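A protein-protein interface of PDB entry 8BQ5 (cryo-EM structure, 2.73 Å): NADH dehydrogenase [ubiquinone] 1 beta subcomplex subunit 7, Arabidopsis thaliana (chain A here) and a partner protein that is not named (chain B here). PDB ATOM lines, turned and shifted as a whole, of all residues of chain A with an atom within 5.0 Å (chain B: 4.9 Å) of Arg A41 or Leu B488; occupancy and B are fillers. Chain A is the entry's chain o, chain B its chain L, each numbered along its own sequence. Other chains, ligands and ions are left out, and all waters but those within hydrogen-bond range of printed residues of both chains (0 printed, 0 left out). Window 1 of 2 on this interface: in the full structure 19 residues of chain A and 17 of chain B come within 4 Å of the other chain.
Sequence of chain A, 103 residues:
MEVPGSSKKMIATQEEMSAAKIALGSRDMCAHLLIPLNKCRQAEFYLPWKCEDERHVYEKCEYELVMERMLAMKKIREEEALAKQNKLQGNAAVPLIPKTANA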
ATOM      1  N   LEU A  34      25.502  -0.225  12.089  1.00  0.00           N
ATOM      2  CA  LEU A  34      24.185  -0.908  11.971  1.00  0.00           C
ATOM      3  C   LEU A  34      23.124  -0.152  12.776  1.00  0.00           C
ATOM      4  O   LEU A  34      21.995  -0.051  12.282  1.00  0.00           O
ATOM      5  CB  LEU A  34      24.331  -2.341  12.487  1.00  0.00           C
ATOM      6  CG  LEU A  34      23.113  -3.242  12.282  1.00  0.00           C
ATOM      7  CD1 LEU A  34      22.620  -3.178  10.844  1.00  0.00           C
ATOM      8  CD2 LEU A  34      23.428  -4.676  12.674  1.00  0.00           C
ATOM      9  N   LEU A  37      21.520   2.509  10.924  1.00  0.00           N
ATOM     10  CA  LEU A  37      20.839   1.926   9.773  1.00  0.00           C
ATOM     11  C   LEU A  37      19.524   1.272  10.183  1.00  0.00           C
ATOM     12  O   LEU A  37      18.505   1.430   9.500  1.00  0.00           O
ATOM     13  CB  LEU A  37      21.753   0.918   9.082  1.00  0.00           C
ATOM     14  CG  LEU A  37      21.097  -0.020   8.070  1.00  0.00           C
ATOM     15  CD1 LEU A  37      20.503   0.761   6.913  1.00  0.00           C
ATOM     16  CD2 LEU A  37      22.111  -1.033   7.570  1.00  0.00           C
ATOM     17  N   ASN A  38      19.526   0.535  11.295  1.00  0.00           N
ATOM     18  CA  ASN A  38      18.288  -0.069  11.776  1.00  0.00           C
ATOM     19  C   ASN A  38      17.329   0.977  12.329  1.00  0.00           C
ATOM     20  O   ASN A  38      16.109   0.789  12.268  1.00  0.00           O
ATOM     21  CB  ASN A  38      18.595  -1.120  12.843  1.00  0.00           C
ATOM     22  CG  ASN A  38      19.028  -2.444  12.250  1.00  0.00           C
ATOM     23  OD1 ASN A  38      19.117  -2.592  11.032  1.00  0.00           O
ATOM     24  ND2 ASN A  38      19.307  -3.416  13.111  1.00  0.00           N
ATOM     25  N   LYS A  39      17.858   2.078  12.866  1.00  0.00           N
ATOM     26  CA  LYS A  39      17.002   3.096  13.468  1.00  0.00           C
ATOM     27  C   LYS A  39      16.094   3.739  12.425  1.00  0.00           C
ATOM     28  O   LYS A  39      14.926   4.036  12.701  1.00  0.00           O
ATOM     29  CB  LYS A  39      17.858   4.150  14.172  1.00  0.00           C
ATOM     30  CG  LYS A  39      17.057   5.261  14.830  1.00  0.00           C
ATOM     31  CD  LYS A  39      17.928   6.469  15.142  1.00  0.00           C
ATOM     32  CE  LYS A  39      17.150   7.768  14.989  1.00  0.00           C
ATOM     33  NZ  LYS A  39      16.783   8.377  16.294  1.00  0.00           N
ATOM     34  N   CYS A  40      16.616   3.967  11.219  1.00  0.00           N
ATOM     35  CA  CYS A  40      15.792   4.544  10.163  1.00  0.00           C
ATOM     36  C   CYS A  40      14.923   3.488   9.496  1.00  0.00           C
ATOM     37  O   CYS A  40      13.826   3.793   9.014  1.00  0.00           O
ATOM     38  CB  CYS A  40      16.670   5.234   9.124  1.00  0.00           C
ATOM     39  SG  CYS A  40      17.570   4.078   8.089  1.00  0.00           S
ATOM     40  N   ARG A  41      15.402   2.241   9.441  1.00  0.00           N
ATOM     41  CA  ARG A  41      14.619   1.182   8.814  1.00  0.00           C
ATOM     42  C   ARG A  41      13.267   1.033   9.495  1.00  0.00           C
ATOM     43  O   ARG A  41      12.230   0.953   8.827  1.00  0.00           O
ATOM     44  CB  ARG A  41      15.393  -0.136   8.847  1.00  0.00           C
ATOM     45  CG  ARG A  41      16.329  -0.323   7.668  1.00  0.00           C
ATOM     46  CD  ARG A  41      16.610  -1.790   7.398  1.00  0.00           C
ATOM     47  NE  ARG A  41      17.732  -2.295   8.179  1.00  0.00           N
ATOM     48  CZ  ARG A  41      18.754  -2.967   7.665  1.00  0.00           C
ATOM     49  NH1 ARG A  41      18.829  -3.227   6.372  1.00  0.00           N
ATOM     50  NH2 ARG A  41      19.726  -3.386   8.471  1.00  0.00           N
ATOM     51  N   GLN A  42      13.259   1.025  10.828  1.00  0.00           N
ATOM     52  CA  GLN A  42      12.001   1.094  11.562  1.00  0.00           C
ATOM     53  C   GLN A  42      11.284   2.412  11.299  1.00  0.00           C
ATOM     54  O   GLN A  42      10.053   2.449  11.203  1.00  0.00           O
ATOM     55  CB  GLN A  42      12.256   0.921  13.058  1.00  0.00           C
ATOM     56  CG  GLN A  42      12.713  -0.467  13.460  1.00  0.00           C
ATOM     57  CD  GLN A  42      12.133  -0.897  14.790  1.00  0.00           C
ATOM     58  OE1 GLN A  42      10.922  -1.082  14.918  1.00  0.00           O
ATOM     59  NE2 GLN A  42      12.991  -1.054  15.790  1.00  0.00           N
ATOM     60  N   ALA A  43      12.041   3.508  11.187  1.00  0.00           N
ATOM     61  CA  ALA A  43      11.424   4.817  11.007  1.00  0.00           C
ATOM     62  C   ALA A  43      10.872   4.999   9.598  1.00  0.00           C
ATOM     63  O   ALA A  43       9.860   5.684   9.416  1.00  0.00           O
ATOM     64  CB  ALA A  43      12.431   5.921  11.330  1.00  0.00           C
ATOM     65  N   GLU A  44      11.516   4.401   8.595  1.00  0.00           N
ATOM     66  CA  GLU A  44      11.106   4.539   7.204  1.00  0.00           C
ATOM     67  C   GLU A  44      10.367   3.310   6.684  1.00  0.00           C
ATOM     68  O   GLU A  44      10.301   3.106   5.466  1.00  0.00           O
ATOM     69  CB  GLU A  44      12.321   4.838   6.324  1.00  0.00           C
ATOM     70  CG  GLU A  44      12.842   6.258   6.459  1.00  0.00           C
ATOM     71  CD  GLU A  44      12.366   7.164   5.339  1.00  0.00           C
ATOM     72  OE1 GLU A  44      13.223   7.735   4.633  1.00  0.00           O
ATOM     73  OE2 GLU A  44      11.138   7.297   5.160  1.00  0.00           O
ATOM     74  N   PHE A  45       9.820   2.489   7.581  1.00  0.00           N
ATOM     75  CA  PHE A  45       9.007   1.326   7.219  1.00  0.00           C
ATOM     76  C   PHE A  45       9.769   0.343   6.334  1.00  0.00           C
ATOM     77  O   PHE A  45       9.182  -0.296   5.459  1.00  0.00           O
ATOM     78  CB  PHE A  45       7.702   1.748   6.535  1.00  0.00           C
ATOM     79  CG  PHE A  45       6.727   2.436   7.445  1.00  0.00           C
ATOM     80  CD1 PHE A  45       5.864   1.703   8.234  1.00  0.00           C
ATOM     81  CD2 PHE A  45       6.658   3.819   7.490  1.00  0.00           C
ATOM     82  CE1 PHE A  45       4.965   2.332   9.066  1.00  0.00           C
ATOM     83  CE2 PHE A  45       5.754   4.455   8.320  1.00  0.00           C
ATOM     84  CZ  PHE A  45       4.904   3.708   9.108  1.00  0.00           C
ATOM     85  N   TYR A  46      11.081   0.221   6.551  1.00  0.00           N
ATOM     86  CA  TYR A  46      11.926  -0.750   5.849  1.00  0.00           C
ATOM     87  C   TYR A  46      11.833  -0.615   4.332  1.00  0.00           C
ATOM     88  O   TYR A  46      11.999  -1.596   3.604  1.00  0.00           O
ATOM     89  CB  TYR A  46      11.586  -2.184   6.260  1.00  0.00           C
ATOM     90  CG  TYR A  46      11.889  -2.519   7.698  1.00  0.00           C
ATOM     91  CD1 TYR A  46      10.967  -2.256   8.700  1.00  0.00           C
ATOM     92  CD2 TYR A  46      13.088  -3.122   8.051  1.00  0.00           C
ATOM     93  CE1 TYR A  46      11.235  -2.569  10.014  1.00  0.00           C
ATOM     94  CE2 TYR A  46      13.365  -3.439   9.363  1.00  0.00           C
ATOM     95  CZ  TYR A  46      12.435  -3.161  10.340  1.00  0.00           C
ATOM     96  OH  TYR A  46      12.706  -3.474  11.650  1.00  0.00           O
ATOM     97  N   CYS A  51      16.949   5.132   3.372  1.00  0.00           N
ATOM     98  CA  CYS A  51      18.187   4.792   4.076  1.00  0.00           C
ATOM     99  C   CYS A  51      19.281   4.283   3.150  1.00  0.00           C
ATOM    100  O   CYS A  51      20.114   3.473   3.565  1.00  0.00           O
ATOM    101  CB  CYS A  51      17.951   3.761   5.183  1.00  0.00           C
ATOM    102  SG  CYS A  51      16.597   4.087   6.306  1.00  0.00           S
ATOM    103  N   ARG A  55      22.584   2.555   4.485  1.00  0.00           N
ATOM    104  CA  ARG A  55      22.769   1.181   4.033  1.00  0.00           C
ATOM    105  C   ARG A  55      24.121   1.000   3.357  1.00  0.00           C
ATOM    106  O   ARG A  55      24.771  -0.039   3.516  1.00  0.00           O
ATOM    107  CB  ARG A  55      21.636   0.792   3.082  1.00  0.00           C
ATOM    108  CG  ARG A  55      21.632  -0.662   2.667  1.00  0.00           C
ATOM    109  CD  ARG A  55      20.337  -1.025   1.956  1.00  0.00           C
ATOM    110  NE  ARG A  55      19.198  -0.297   2.501  1.00  0.00           N
ATOM    111  CZ  ARG A  55      18.119   0.036   1.805  1.00  0.00           C
ATOM    112  NH1 ARG A  55      17.989  -0.299   0.532  1.00  0.00           N
ATOM    113  NH2 ARG A  55      17.150   0.724   2.400  1.00  0.00           N
ATOM    114  N   TYR A  58      27.130   0.817   5.783  1.00  0.00           N
ATOM    115  CA  TYR A  58      27.148  -0.466   6.474  1.00  0.00           C
ATOM    116  C   TYR A  58      27.578  -1.587   5.538  1.00  0.00           C
ATOM    117  O   TYR A  58      28.390  -2.440   5.913  1.00  0.00           O
ATOM    118  CB  TYR A  58      25.775  -0.770   7.072  1.00  0.00           C
ATOM    119  CG  TYR A  58      25.705  -2.125   7.738  1.00  0.00           C
ATOM    120  CD1 TYR A  58      26.213  -2.311   9.014  1.00  0.00           C
ATOM    121  CD2 TYR A  58      25.137  -3.214   7.092  1.00  0.00           C
ATOM    122  CE1 TYR A  58      26.158  -3.540   9.632  1.00  0.00           C
ATOM    123  CE2 TYR A  58      25.076  -4.453   7.705  1.00  0.00           C
ATOM    124  CZ  TYR A  58      25.589  -4.608   8.976  1.00  0.00           C
ATOM    125  OH  TYR A  58      25.537  -5.832   9.599  1.00  0.00           O
ATOM    126  N   GLU A  59      27.045  -1.606   4.314  1.00  0.00           N
ATOM    127  CA  GLU A  59      27.425  -2.655   3.375  1.00  0.00           C
ATOM    128  C   GLU A  59      28.895  -2.549   2.993  1.00  0.00           C
ATOM    129  O   GLU A  59      29.544  -3.564   2.719  1.00  0.00           O
ATOM    130  CB  GLU A  59      26.545  -2.615   2.128  1.00  0.00           C
ATOM    131  CG  GLU A  59      25.103  -3.034   2.352  1.00  0.00           C
ATOM    132  CD  GLU A  59      24.349  -3.170   1.047  1.00  0.00           C
ATOM    133  OE1 GLU A  59      23.158  -2.802   0.995  1.00  0.00           O
ATOM    134  OE2 GLU A  59      24.953  -3.658   0.069  1.00  0.00           O
ATOM    135  N   GLU A  62      30.683  -4.456   5.857  1.00  0.00           N
ATOM    136  CA  GLU A  62      30.591  -5.906   5.915  1.00  0.00           C
ATOM    137  C   GLU A  62      31.316  -6.530   4.734  1.00  0.00           C
ATOM    138  O   GLU A  62      31.674  -7.713   4.766  1.00  0.00           O
ATOM    139  CB  GLU A  62      29.125  -6.328   5.961  1.00  0.00           C
ATOM    140  CG  GLU A  62      28.858  -7.586   6.782  1.00  0.00           C
ATOM    141  CD  GLU A  62      29.164  -7.418   8.263  1.00  0.00           C
ATOM    142  OE1 GLU A  62      28.253  -7.017   9.018  1.00  0.00           O
ATOM    143  OE2 GLU A  62      30.307  -7.706   8.675  1.00  0.00           O
ATOM    144  N   ASP B 483      14.745  -5.935   1.508  1.00  0.00           N
ATOM    145  CA  ASP B 483      15.484  -5.341   2.618  1.00  0.00           C
ATOM    146  C   ASP B 483      14.821  -5.659   3.949  1.00  0.00           C
ATOM    147  O   ASP B 483      15.496  -5.793   4.976  1.00  0.00           O
ATOM    148  CB  ASP B 483      15.607  -3.829   2.432  1.00  0.00           C
ATOM    149  CG  ASP B 483      16.710  -3.228   3.283  1.00  0.00           C
ATOM    150  OD1 ASP B 483      17.797  -3.836   3.366  1.00  0.00           O
ATOM    151  OD2 ASP B 483      16.484  -2.156   3.883  1.00  0.00           O
ATOM    152  N   ILE B 486      15.499 -10.041   4.371  1.00  0.00           N
ATOM    153  CA  ILE B 486      16.839 -10.595   4.214  1.00  0.00           C
ATOM    154  C   ILE B 486      17.917  -9.530   4.093  1.00  0.00           C
ATOM    155  O   ILE B 486      19.067  -9.864   3.804  1.00  0.00           O
ATOM    156  CB  ILE B 486      16.913 -11.557   3.010  1.00  0.00           C
ATOM    157  CG1 ILE B 486      16.872 -10.772   1.697  1.00  0.00           C
ATOM    158  CG2 ILE B 486      15.794 -12.589   3.080  1.00  0.00           C
ATOM    159  CD1 ILE B 486      16.538 -11.610   0.491  1.00  0.00           C
ATOM    160  N   GLY B 487      17.589  -8.256   4.299  1.00  0.00           N
ATOM    161  CA  GLY B 487      18.598  -7.215   4.298  1.00  0.00           C
ATOM    162  C   GLY B 487      19.675  -7.473   5.331  1.00  0.00           C
ATOM    163  O   GLY B 487      19.374  -7.911   6.444  1.00  0.00           O
ATOM    164  N   LEU B 488      20.931  -7.225   4.968  1.00  0.00           N
ATOM    165  CA  LEU B 488      22.052  -7.492   5.861  1.00  0.00           C
ATOM    166  C   LEU B 488      21.867  -6.795   7.199  1.00  0.00           C
ATOM    167  O   LEU B 488      21.860  -5.562   7.275  1.00  0.00           O
ATOM    168  CB  LEU B 488      23.357  -7.040   5.201  1.00  0.00           C
ATOM    169  CG  LEU B 488      24.594  -7.904   5.443  1.00  0.00           C
ATOM    170  CD1 LEU B 488      24.394  -9.292   4.872  1.00  0.00           C
ATOM    171  CD2 LEU B 488      25.820  -7.251   4.831  1.00  0.00           C
ATOM    172  N   GLY B 489      21.706  -7.593   8.253  1.00  0.00           N
ATOM    173  CA  GLY B 489      21.553  -7.082   9.598  1.00  0.00           C
ATOM    174  C   GLY B 489      20.168  -6.603   9.970  1.00  0.00           C
ATOM    175  O   GLY B 489      20.008  -6.021  11.048  1.00  0.00           O
ATOM    176  N   THR B 490      19.166  -6.828   9.122  1.00  0.00           N
ATOM    177  CA  THR B 490      17.831  -6.310   9.396  1.00  0.00           C
ATOM    178  C   THR B 490      17.274  -6.894  10.690  1.00  0.00           C
ATOM    179  O   THR B 490      17.464  -8.074  10.998  1.00  0.00           O
ATOM    180  CB  THR B 490      16.888  -6.602   8.221  1.00  0.00           C
ATOM    181  OG1 THR B 490      15.630  -5.950   8.439  1.00  0.00           O
ATOM    182  CG2 THR B 490      16.657  -8.098   8.050  1.00  0.00           C
ATOM    183  N   LEU B 506      25.417 -14.905   5.411  1.00  0.00           N
ATOM    184  CA  LEU B 506      24.787 -14.036   4.421  1.00  0.00           C
ATOM    185  C   LEU B 506      25.789 -13.054   3.827  1.00  0.00           C
ATOM    186  O   LEU B 506      25.815 -12.836   2.611  1.00  0.00           O
ATOM    187  CB  LEU B 506      23.610 -13.296   5.053  1.00  0.00           C
ATOM    188  CG  LEU B 506      22.724 -12.486   4.107  1.00  0.00           C
ATOM    189  CD1 LEU B 506      22.083 -13.389   3.070  1.00  0.00           C
ATOM    190  CD2 LEU B 506      21.661 -11.750   4.899  1.00  0.00           C
ATOM    191  N   ALA B 507      26.623 -12.448   4.676  1.00  0.00           N
ATOM    192  CA  ALA B 507      27.600 -11.478   4.189  1.00  0.00           C
ATOM    193  C   ALA B 507      28.546 -12.112   3.179  1.00  0.00           C
ATOM    194  O   ALA B 507      28.745 -11.585   2.079  1.00  0.00           O
ATOM    195  CB  ALA B 507      28.383 -10.890   5.364  1.00  0.00           C
ATOM    196  N   GLU B 510      27.092 -12.730  -0.413  1.00  0.00           N
ATOM    197  CA  GLU B 510      26.927 -11.607  -1.328  1.00  0.00           C
ATOM    198  C   GLU B 510      28.221 -10.849  -1.601  1.00  0.00           C
ATOM    199  O   GLU B 510      28.204  -9.911  -2.404  1.00  0.00           O
ATOM    200  CB  GLU B 510      25.867 -10.638  -0.786  1.00  0.00           C
ATOM    201  CG  GLU B 510      26.299  -9.834   0.436  1.00  0.00           C
ATOM    202  CD  GLU B 510      25.422  -8.615   0.679  1.00  0.00           C
ATOM    203  OE1 GLU B 510      25.060  -7.928  -0.299  1.00  0.00           O
ATOM    204  OE2 GLU B 510      25.091  -8.344   1.851  1.00  0.00           O
ATOM    205  N   PHE B 511      29.335 -11.225  -0.972  1.00  0.00           N
ATOM    206  CA  PHE B 511      30.574 -10.473  -1.142  1.00  0.00           C
ATOM    207  C   PHE B 511      31.739 -11.362  -1.562  1.00  0.00           C
ATOM    208  O   PHE B 511      32.622 -10.923  -2.306  1.00  0.00           O
ATOM    209  CB  PHE B 511      30.933  -9.736   0.149  1.00  0.00           C
ATOM    210  CG  PHE B 511      29.939  -8.682   0.546  1.00  0.00           C
ATOM    211  CD1 PHE B 511      29.421  -7.807  -0.392  1.00  0.00           C
ATOM    212  CD2 PHE B 511      29.534  -8.560   1.864  1.00  0.00           C
ATOM    213  CE1 PHE B 511      28.511  -6.837  -0.024  1.00  0.00           C
ATOM    214  CE2 PHE B 511      28.625  -7.592   2.237  1.00  0.00           C
ATOM    215  CZ  PHE B 511      28.114  -6.728   1.290  1.00  0.00           C
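OD1 of Asp B483 lies within salt-bridge range of NH1 of Arg A41 (3.2 Å).
The side-chain carboxylate (OD2) of Asp B483 lies within salt-bridge range of the guanidinium group (NH2) of Arg A55 (3.3 Å).
O of Leu B488 sits at hydrogen-bond distance from NH2 of Arg A41 (3.3 Å).
The side-chain amide nitrogen of Asn A38 lies within hydrogen-bond range of the backbone carbonyl oxygen of Gly B489 (3.4 Å).
The backbone carbonyl oxygen (O) of Asp B483 is in hydrogen-bond range of the side-chain hydroxyl (OG1) of Thr B490.
NH2 of Arg A41 lies within hydrogen-bond range of OD1 of Asn A38, at 2.7 Å.
O of Arg A41 lies within hydrogen-bond range of N of Tyr A46 (2.7 Å).
The side-chain carboxylate (OE1) of Glu A62 lies within hydrogen-bond range of the side-chain hydroxyl (OH) of Tyr A58 (3.0 Å).
The side-chain sulfur (SG) of Cys A40 is disulfide-bonded to the side-chain sulfur (SG) of Cys A51.
Gly B489 touches Leu A34 (O to CD1, 3.9 Å).
Arg A41 touches Gly B489.
NH2 of Arg A41 touches N of Thr B490 (3.5 Å).
Tyr A46 touches Thr B490.
O of Leu B488 touches CE2 of Tyr A58 (3.4 Å).
Phe B511 touches Glu A59 (CZ to O, 3.8 Å).
Glu A62 touches Leu B488 (CB to CD2, 3.6 Å).
Glu A62 touches Ala B507 (CG to CB, 3.6 Å).
Phe B511 touches Glu A62 (CD2 to O, 3.7 Å).
Arg A41 touches just these residues of chain B: Asp B483, Leu B488, Gly B489 and Thr B490.
Of the printed residues of chain A, Phe B511 touches Glu A59 and Glu A62.
Printed residues of chain B within 4 Å of Glu A62: Leu B488, Ala B507 and Phe B511.
Of the printed residues of chain B, Tyr A58 touches Leu B488 (3.4 Å).
The nearest residue of chain B that does not touch Arg A41 is Gly B487 (4.5 Å).
The nearest residue of chain A that does not touch Leu B488 is Leu A34 (4.4 Å).
The nearest printed residue of chain A that does not touch Phe B511 is Tyr A58 (6.3 Å).
Of the 10 printed residues of chain B, 6 touch a printed residue of chain A.
Printed residues of chain B that touch a printed residue of chain A: Asp B483, Leu B488, Gly B489, Thr B490, Ala B507 and Phe B511.
Hydrophobic or aromatic side chains of chain B within 4 Å of the printed part of chain A: Leu B488, Ala B507 and Phe B511.
Hydrophobic or aromatic side chains of chain A that line the printed part of chain B: Leu A34, Tyr A46 and Tyr A58.
Among the printed residues, Asp or Glu carboxylates within 4 Å of a Lys or Arg side-chain nitrogen of the other chain: Arg A41 with Asp B483 (3.2 Å) and Arg A55 with Asp B483 (3.3 Å).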
